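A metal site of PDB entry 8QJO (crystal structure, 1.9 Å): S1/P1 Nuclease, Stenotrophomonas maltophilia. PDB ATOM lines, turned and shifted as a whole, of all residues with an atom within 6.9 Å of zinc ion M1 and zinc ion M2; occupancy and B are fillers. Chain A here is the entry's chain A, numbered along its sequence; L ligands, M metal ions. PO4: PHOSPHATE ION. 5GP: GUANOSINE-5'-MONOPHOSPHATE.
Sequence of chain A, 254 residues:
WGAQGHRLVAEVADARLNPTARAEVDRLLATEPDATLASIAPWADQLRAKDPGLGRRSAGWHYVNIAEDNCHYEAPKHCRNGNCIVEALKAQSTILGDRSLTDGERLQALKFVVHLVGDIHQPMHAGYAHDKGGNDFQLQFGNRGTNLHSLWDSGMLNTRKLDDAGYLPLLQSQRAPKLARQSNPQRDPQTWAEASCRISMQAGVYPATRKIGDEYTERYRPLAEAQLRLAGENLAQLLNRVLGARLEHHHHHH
O1P of 5GP L2 is in salt-bridge range of NE of Arg 48, 3.9 Å away.
A ring nitrogen (ND1) of His 6 sits close to a ring nitrogen (ND1) of His 115 (3.4 Å).
A ring nitrogen (ND1) of His 62 lies close to the guanidinium group (NH1) of Arg 48, at 3.4 Å.
The backbone carbonyl oxygen (O) of His 62 sits at hydrogen-bond distance from a ring nitrogen (ND1) of His 125, 2.7 Å away.
NE1 of Trp 1 is in hydrogen-bond range of O of Gly 118.
The side-chain carboxylate of Asp 45 sits close to the guanidinium group of Arg 48 (3.3 Å).
Arg 48 touches zinc ion M1.
Within 4 Å of zinc ion M1: Asp 45, Arg 48, His 62, His 115 and Asp 119.
The nearest printed residue that does not touch zinc ion M1 is His 6 (4.2 Å).
Within 4 Å of zinc ion M2: Trp 1, His 6, Asp 45 and Asp 119.
Zinc ion M1 is bound by a ring nitrogen (NE2) of His 115 (2.1 Å), the side-chain carboxylate of Asp 119 (2.1 Å), a ring nitrogen (ND1) of His 62 (2.1 Å), an oxygen (O4) of PO4 L1 (2.2 Å), an oxygen (O3) of PO4 L1 (2.3 Å) and the side-chain carboxylate of Asp 45 (2.5 Å).
Zinc ion M2 is bound by O3 of PO4 L1 (1.9 Å), NE2 of His 6 (2.0 Å), OD1 of Asp 119 (2.1 Å), O of Trp 1 (2.2 Å) and N of Trp 1 (2.2 Å).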
ATOM      1  N   TRP A   1     -13.302   4.673  -3.906  1.00  0.00           N
ATOM      2  CA  TRP A   1     -12.008   4.097  -4.316  1.00  0.00           C
ATOM      3  C   TRP A   1     -12.030   2.570  -4.150  1.00  0.00           C
ATOM      4  O   TRP A   1     -12.800   2.081  -3.336  1.00  0.00           O
ATOM      5  CB  TRP A   1     -10.818   4.703  -3.528  1.00  0.00           C
ATOM      6  CG  TRP A   1     -10.827   6.190  -3.440  1.00  0.00           C
ATOM      7  CD1 TRP A   1     -11.221   6.955  -2.381  1.00  0.00           C
ATOM      8  CD2 TRP A   1     -10.474   7.118  -4.486  1.00  0.00           C
ATOM      9  NE1 TRP A   1     -11.150   8.282  -2.701  1.00  0.00           N
ATOM     10  CE2 TRP A   1     -10.663   8.419  -3.984  1.00  0.00           C
ATOM     11  CE3 TRP A   1      -9.977   6.963  -5.783  1.00  0.00           C
ATOM     12  CZ2 TRP A   1     -10.424   9.560  -4.726  1.00  0.00           C
ATOM     13  CZ3 TRP A   1      -9.717   8.095  -6.527  1.00  0.00           C
ATOM     14  CH2 TRP A   1      -9.945   9.375  -6.011  1.00  0.00           C
ATOM     15  N   GLY A   2     -11.146   1.907  -4.861  1.00  0.00           N
ATOM     16  CA  GLY A   2     -10.735   0.515  -4.612  1.00  0.00           C
ATOM     17  C   GLY A   2      -9.953   0.440  -3.329  1.00  0.00           C
ATOM     18  O   GLY A   2      -9.731   1.519  -2.720  1.00  0.00           O
ATOM     19  N   ALA A   3      -9.547  -0.766  -2.921  1.00  0.00           N
ATOM     20  CA  ALA A   3      -8.947  -1.044  -1.600  1.00  0.00           C
ATOM     21  C   ALA A   3      -7.675  -0.181  -1.428  1.00  0.00           C
ATOM     22  O   ALA A   3      -7.513   0.402  -0.337  1.00  0.00           O
ATOM     23  CB  ALA A   3      -8.679  -2.526  -1.454  1.00  0.00           C
ATOM     24  N   GLY A   5      -6.762   2.787  -2.804  1.00  0.00           N
ATOM     25  CA  GLY A   5      -7.123   4.201  -2.597  1.00  0.00           C
ATOM     26  C   GLY A   5      -7.536   4.447  -1.153  1.00  0.00           C
ATOM     27  O   GLY A   5      -7.075   5.420  -0.579  1.00  0.00           O
ATOM     28  N   HIS A   6      -8.358   3.566  -0.588  1.00  0.00           N
ATOM     29  CA  HIS A   6      -8.794   3.623   0.830  1.00  0.00           C
ATOM     30  C   HIS A   6      -7.579   3.582   1.770  1.00  0.00           C
ATOM     31  O   HIS A   6      -7.542   4.399   2.756  1.00  0.00           O
ATOM     32  CB  HIS A   6      -9.876   2.561   1.108  1.00  0.00           C
ATOM     33  CG  HIS A   6     -11.177   3.027   0.542  1.00  0.00           C
ATOM     34  ND1 HIS A   6     -11.846   4.101   1.081  1.00  0.00           N
ATOM     35  CD2 HIS A   6     -11.862   2.650  -0.546  1.00  0.00           C
ATOM     36  CE1 HIS A   6     -12.955   4.309   0.380  1.00  0.00           C
ATOM     37  NE2 HIS A   6     -12.959   3.467  -0.663  1.00  0.00           N
ATOM     38  N   PRO A  42     -10.631  -0.314   3.815  1.00  0.00           N
ATOM     39  CA  PRO A  42     -11.564  -0.956   2.885  1.00  0.00           C
ATOM     40  C   PRO A  42     -12.757  -1.719   3.500  1.00  0.00           C
ATOM     41  O   PRO A  42     -13.643  -2.142   2.753  1.00  0.00           O
ATOM     42  CB  PRO A  42     -10.677  -1.970   2.113  1.00  0.00           C
ATOM     43  CG  PRO A  42      -9.274  -1.518   2.419  1.00  0.00           C
ATOM     44  CD  PRO A  42      -9.355  -1.051   3.859  1.00  0.00           C
ATOM     45  N   ALA A  44     -15.675  -1.357   5.021  1.00  0.00           N
ATOM     46  CA  ALA A  44     -17.092  -1.048   4.686  1.00  0.00           C
ATOM     47  C   ALA A  44     -17.490  -1.647   3.335  1.00  0.00           C
ATOM     48  O   ALA A  44     -18.669  -2.003   3.185  1.00  0.00           O
ATOM     49  CB  ALA A  44     -17.292   0.447   4.739  1.00  0.00           C
ATOM     50  N   ASP A  45     -16.561  -1.771   2.377  1.00  0.00           N
ATOM     51  CA  ASP A  45     -16.830  -2.378   1.034  1.00  0.00           C
ATOM     52  C   ASP A  45     -16.956  -3.902   1.174  1.00  0.00           C
ATOM     53  O   ASP A  45     -17.790  -4.467   0.467  1.00  0.00           O
ATOM     54  CB  ASP A  45     -15.763  -2.060  -0.014  1.00  0.00           C
ATOM     55  CG  ASP A  45     -15.778  -0.628  -0.499  1.00  0.00           C
ATOM     56  OD1 ASP A  45     -16.859   0.049  -0.370  1.00  0.00           O
ATOM     57  OD2 ASP A  45     -14.711  -0.198  -0.995  1.00  0.00           O
ATOM     58  N   ARG A  48     -20.339  -4.426   2.822  1.00  0.00           N
ATOM     59  CA  ARG A  48     -21.355  -4.276   1.747  1.00  0.00           C
ATOM     60  C   ARG A  48     -21.469  -5.581   0.941  1.00  0.00           C
ATOM     61  O   ARG A  48     -22.579  -5.982   0.623  1.00  0.00           O
ATOM     62  CB  ARG A  48     -21.013  -3.138   0.776  1.00  0.00           C
ATOM     63  CG  ARG A  48     -22.105  -2.883  -0.249  1.00  0.00           C
ATOM     64  CD  ARG A  48     -21.765  -1.824  -1.282  1.00  0.00           C
ATOM     65  NE  ARG A  48     -20.455  -2.078  -1.887  1.00  0.00           N
ATOM     66  CZ  ARG A  48     -19.568  -1.160  -2.230  1.00  0.00           C
ATOM     67  NH1 ARG A  48     -19.795   0.160  -2.089  1.00  0.00           N
ATOM     68  NH2 ARG A  48     -18.424  -1.579  -2.752  1.00  0.00           N
ATOM     69  N   ALA A  59     -25.227   0.230   1.946  1.00  0.00           N
ATOM     70  CA  ALA A  59     -24.711   0.353   0.563  1.00  0.00           C
ATOM     71  C   ALA A  59     -24.835   1.801   0.096  1.00  0.00           C
ATOM     72  O   ALA A  59     -23.856   2.327  -0.449  1.00  0.00           O
ATOM     73  CB  ALA A  59     -25.423  -0.565  -0.415  1.00  0.00           C
ATOM     74  N   TRP A  61     -24.716   4.414   1.792  1.00  0.00           N
ATOM     75  CA  TRP A  61     -23.840   5.323   2.598  1.00  0.00           C
ATOM     76  C   TRP A  61     -22.551   5.676   1.826  1.00  0.00           C
ATOM     77  O   TRP A  61     -21.856   6.579   2.287  1.00  0.00           O
ATOM     78  CB  TRP A  61     -23.477   4.731   3.957  1.00  0.00           C
ATOM     79  CG  TRP A  61     -24.620   4.352   4.850  1.00  0.00           C
ATOM     80  CD1 TRP A  61     -25.962   4.373   4.597  1.00  0.00           C
ATOM     81  CD2 TRP A  61     -24.485   3.837   6.184  1.00  0.00           C
ATOM     82  NE1 TRP A  61     -26.658   3.942   5.690  1.00  0.00           N
ATOM     83  CE2 TRP A  61     -25.774   3.583   6.668  1.00  0.00           C
ATOM     84  CE3 TRP A  61     -23.381   3.541   6.999  1.00  0.00           C
ATOM     85  CZ2 TRP A  61     -26.001   3.067   7.936  1.00  0.00           C
ATOM     86  CZ3 TRP A  61     -23.602   3.028   8.251  1.00  0.00           C
ATOM     87  CH2 TRP A  61     -24.898   2.796   8.712  1.00  0.00           C
ATOM     88  N   HIS A  62     -22.220   4.986   0.733  1.00  0.00           N
ATOM     89  CA  HIS A  62     -20.917   5.175   0.016  1.00  0.00           C
ATOM     90  C   HIS A  62     -20.972   6.348  -0.944  1.00  0.00           C
ATOM     91  O   HIS A  62     -19.897   6.807  -1.388  1.00  0.00           O
ATOM     92  CB  HIS A  62     -20.461   3.877  -0.667  1.00  0.00           C
ATOM     93  CG  HIS A  62     -20.172   2.780   0.324  1.00  0.00           C
ATOM     94  ND1 HIS A  62     -18.945   2.199   0.462  1.00  0.00           N
ATOM     95  CD2 HIS A  62     -20.975   2.188   1.234  1.00  0.00           C
ATOM     96  CE1 HIS A  62     -19.008   1.282   1.399  1.00  0.00           C
ATOM     97  NE2 HIS A  62     -20.246   1.247   1.893  1.00  0.00           N
ATOM     98  N   TYR A  63     -22.157   6.861  -1.264  1.00  0.00           N
ATOM     99  CA  TYR A  63     -22.311   7.849  -2.348  1.00  0.00           C
ATOM    100  C   TYR A  63     -23.487   8.780  -2.079  1.00  0.00           C
ATOM    101  O   TYR A  63     -24.257   8.630  -1.101  1.00  0.00           O
ATOM    102  CB  TYR A  63     -22.418   7.123  -3.702  1.00  0.00           C
ATOM    103  CG  TYR A  63     -23.627   6.236  -3.809  1.00  0.00           C
ATOM    104  CD1 TYR A  63     -24.873   6.763  -4.127  1.00  0.00           C
ATOM    105  CD2 TYR A  63     -23.536   4.883  -3.543  1.00  0.00           C
ATOM    106  CE1 TYR A  63     -25.999   5.957  -4.214  1.00  0.00           C
ATOM    107  CE2 TYR A  63     -24.658   4.073  -3.617  1.00  0.00           C
ATOM    108  CZ  TYR A  63     -25.891   4.612  -3.959  1.00  0.00           C
ATOM    109  OH  TYR A  63     -26.987   3.802  -4.018  1.00  0.00           O
ATOM    110  N   ILE A  85     -23.937   9.302   1.786  1.00  0.00           N
ATOM    111  CA  ILE A  85     -22.590   9.477   2.383  1.00  0.00           C
ATOM    112  C   ILE A  85     -22.566  10.757   3.235  1.00  0.00           C
ATOM    113  O   ILE A  85     -21.906  10.715   4.251  1.00  0.00           O
ATOM    114  CB  ILE A  85     -21.506   9.445   1.316  1.00  0.00           C
ATOM    115  CG1 ILE A  85     -20.123   9.282   1.978  1.00  0.00           C
ATOM    116  CG2 ILE A  85     -21.591  10.670   0.420  1.00  0.00           C
ATOM    117  CD1 ILE A  85     -19.060   8.794   1.004  1.00  0.00           C
ATOM    118  N   HIS A 115     -13.401   5.081   5.831  1.00  0.00           N
ATOM    119  CA  HIS A 115     -13.849   4.689   4.474  1.00  0.00           C
ATOM    120  C   HIS A 115     -14.542   5.870   3.782  1.00  0.00           C
ATOM    121  O   HIS A 115     -14.222   6.148   2.621  1.00  0.00           O
ATOM    122  CB  HIS A 115     -14.823   3.513   4.551  1.00  0.00           C
ATOM    123  CG  HIS A 115     -15.102   2.959   3.205  1.00  0.00           C
ATOM    124  ND1 HIS A 115     -14.203   2.117   2.582  1.00  0.00           N
ATOM    125  CD2 HIS A 115     -16.127   3.177   2.348  1.00  0.00           C
ATOM    126  CE1 HIS A 115     -14.671   1.804   1.379  1.00  0.00           C
ATOM    127  NE2 HIS A 115     -15.846   2.484   1.200  1.00  0.00           N
ATOM    128  N   LEU A 116     -15.496   6.501   4.476  1.00  0.00           N
ATOM    129  CA  LEU A 116     -16.432   7.483   3.890  1.00  0.00           C
ATOM    130  C   LEU A 116     -15.712   8.805   3.647  1.00  0.00           C
ATOM    131  O   LEU A 116     -16.085   9.461   2.690  1.00  0.00           O
ATOM    132  CB  LEU A 116     -17.651   7.683   4.797  1.00  0.00           C
ATOM    133  CG  LEU A 116     -18.551   6.468   4.907  1.00  0.00           C
ATOM    134  CD1 LEU A 116     -19.774   6.733   5.766  1.00  0.00           C
ATOM    135  CD2 LEU A 116     -18.945   5.994   3.530  1.00  0.00           C
ATOM    136  N   GLY A 118     -12.687   8.865   2.567  1.00  0.00           N
ATOM    137  CA  GLY A 118     -12.133   8.402   1.274  1.00  0.00           C
ATOM    138  C   GLY A 118     -13.135   8.548   0.148  1.00  0.00           C
ATOM    139  O   GLY A 118     -12.900   9.294  -0.798  1.00  0.00           O
ATOM    140  N   ASP A 119     -14.253   7.835   0.234  1.00  0.00           N
ATOM    141  CA  ASP A 119     -15.294   7.803  -0.810  1.00  0.00           C
ATOM    142  C   ASP A 119     -15.835   9.199  -1.100  1.00  0.00           C
ATOM    143  O   ASP A 119     -16.091   9.464  -2.245  1.00  0.00           O
ATOM    144  CB  ASP A 119     -16.436   6.862  -0.436  1.00  0.00           C
ATOM    145  CG  ASP A 119     -16.172   5.399  -0.834  1.00  0.00           C
ATOM    146  OD1 ASP A 119     -15.123   5.129  -1.458  1.00  0.00           O
ATOM    147  OD2 ASP A 119     -17.024   4.566  -0.516  1.00  0.00           O
ATOM    148  N   GLN A 122     -14.005  10.874  -3.822  1.00  0.00           N
ATOM    149  CA  GLN A 122     -13.978  10.255  -5.164  1.00  0.00           C
ATOM    150  C   GLN A 122     -15.058  10.973  -5.969  1.00  0.00           C
ATOM    151  O   GLN A 122     -16.248  10.881  -5.640  1.00  0.00           O
ATOM    152  CB  GLN A 122     -14.141   8.740  -5.041  1.00  0.00           C
ATOM    153  CG  GLN A 122     -13.486   7.895  -6.134  1.00  0.00           C
ATOM    154  CD  GLN A 122     -14.235   7.928  -7.441  1.00  0.00           C
ATOM    155  OE1 GLN A 122     -14.377   8.975  -8.054  1.00  0.00           O
ATOM    156  NE2 GLN A 122     -14.748   6.770  -7.876  1.00  0.00           N
ATOM    157  N   HIS A 125     -18.420   9.335  -6.765  1.00  0.00           N
ATOM    158  CA  HIS A 125     -19.255   9.053  -5.565  1.00  0.00           C
ATOM    159  C   HIS A 125     -20.233  10.217  -5.261  1.00  0.00           C
ATOM    160  O   HIS A 125     -21.039  10.112  -4.296  1.00  0.00           O
ATOM    161  CB  HIS A 125     -18.346   8.675  -4.416  1.00  0.00           C
ATOM    162  CG  HIS A 125     -17.917   7.247  -4.455  1.00  0.00           C
ATOM    163  ND1 HIS A 125     -18.243   6.356  -3.453  1.00  0.00           N
ATOM    164  CD2 HIS A 125     -17.154   6.546  -5.331  1.00  0.00           C
ATOM    165  CE1 HIS A 125     -17.734   5.175  -3.739  1.00  0.00           C
ATOM    166  NE2 HIS A 125     -17.070   5.260  -4.872  1.00  0.00           N
ATOM    167  N   HIS A 149     -16.950   4.747 -13.415  1.00  0.00           N
ATOM    168  CA  HIS A 149     -16.850   4.637 -11.931  1.00  0.00           C
ATOM    169  C   HIS A 149     -15.573   3.875 -11.570  1.00  0.00           C
ATOM    170  O   HIS A 149     -14.783   4.390 -10.770  1.00  0.00           O
ATOM    171  CB  HIS A 149     -18.092   4.010 -11.282  1.00  0.00           C
ATOM    172  CG  HIS A 149     -18.058   4.156  -9.791  1.00  0.00           C
ATOM    173  ND1 HIS A 149     -18.702   5.199  -9.146  1.00  0.00           N
ATOM    174  CD2 HIS A 149     -17.425   3.436  -8.840  1.00  0.00           C
ATOM    175  CE1 HIS A 149     -18.516   5.076  -7.842  1.00  0.00           C
ATOM    176  NE2 HIS A 149     -17.685   4.041  -7.625  1.00  0.00           N
ATOM    177  N   ASP A 153     -12.300   4.796  -9.364  1.00  0.00           N
ATOM    178  CA  ASP A 153     -12.063   3.947  -8.172  1.00  0.00           C
ATOM    179  C   ASP A 153     -10.645   3.399  -8.157  1.00  0.00           C
ATOM    180  O   ASP A 153     -10.000   3.473  -7.071  1.00  0.00           O
ATOM    181  CB  ASP A 153     -13.076   2.801  -8.027  1.00  0.00           C
ATOM    182  CG  ASP A 153     -14.308   3.180  -7.232  1.00  0.00           C
ATOM    183  OD1 ASP A 153     -14.328   4.340  -6.657  1.00  0.00           O
ATOM    184  OD2 ASP A 153     -15.195   2.306  -7.108  1.00  0.00           O
HETATM  185  P   PO4 L   1     -16.449   1.832  -3.114  1.00  0.00           P
HETATM  186  O1  PO4 L   1     -16.430   0.386  -3.580  1.00  0.00           O
HETATM  187  O2  PO4 L   1     -16.113   2.711  -4.270  1.00  0.00           O
HETATM  188  O3  PO4 L   1     -15.385   2.024  -2.014  1.00  0.00           O
HETATM  189  O4  PO4 L   1     -17.783   2.182  -2.557  1.00  0.00           O
HETATM  190  P   5GP L   2     -21.912  -1.567  -6.838  1.00  0.00           P
HETATM  191  O1P 5GP L   2     -21.046  -2.080  -5.714  1.00  0.00           O
HETATM  192  O2P 5GP L   2     -21.872  -2.333  -8.160  1.00  0.00           O
HETATM  193  O3P 5GP L   2     -23.381  -1.320  -6.391  1.00  0.00           O
HETATM  194  O5' 5GP L   2     -21.336  -0.055  -7.238  1.00  0.00           O
HETATM  195  C5' 5GP L   2     -19.972   0.128  -7.621  1.00  0.00           C
HETATM  196  C4' 5GP L   2     -19.526   1.457  -7.081  1.00  0.00           C
HETATM  197  O4' 5GP L   2     -20.459   2.469  -7.504  1.00  0.00           O
HETATM  198  C3' 5GP L   2     -19.407   1.578  -5.557  1.00  0.00           C
HETATM  199  O3' 5GP L   2     -18.246   2.324  -5.205  1.00  0.00           O
HETATM  200  C2' 5GP L   2     -20.746   2.220  -5.158  1.00  0.00           C
HETATM  201  O2' 5GP L   2     -20.645   3.061  -4.015  1.00  0.00           O
HETATM  202  C1' 5GP L   2     -21.042   3.105  -6.374  1.00  0.00           C
HETATM  203  N9  5GP L   2     -22.460   3.316  -6.676  1.00  0.00           N
HETATM  204  C8  5GP L   2     -23.504   2.414  -6.796  1.00  0.00           C
HETATM  205  N7  5GP L   2     -24.629   2.970  -7.223  1.00  0.00           N
HETATM  206  C5  5GP L   2     -24.310   4.319  -7.340  1.00  0.00           C
HETATM  207  C6  5GP L   2     -25.123   5.445  -7.605  1.00  0.00           C
HETATM  208  O6  5GP L   2     -26.338   5.441  -7.792  1.00  0.00           O
HETATM  209  N1  5GP L   2     -24.428   6.636  -7.507  1.00  0.00           N
HETATM  210  C2  5GP L   2     -23.076   6.748  -7.202  1.00  0.00           C
HETATM  211  N2  5GP L   2     -22.566   7.995  -7.157  1.00  0.00           N
HETATM  212  N3  5GP L   2     -22.294   5.693  -6.943  1.00  0.00           N
HETATM  213  C4  5GP L   2     -22.961   4.539  -7.024  1.00  0.00           C
HETATM  214 ZN    ZN M   1     -17.068   2.491  -0.469  1.00  0.00          ZN
HETATM  215 ZN    ZN M   2     -14.108   3.449  -2.272  1.00  0.00          ZN
HETATM  216 ZN    ZN M   3     -16.634   3.599  -5.929  1.00  0.00          ZN
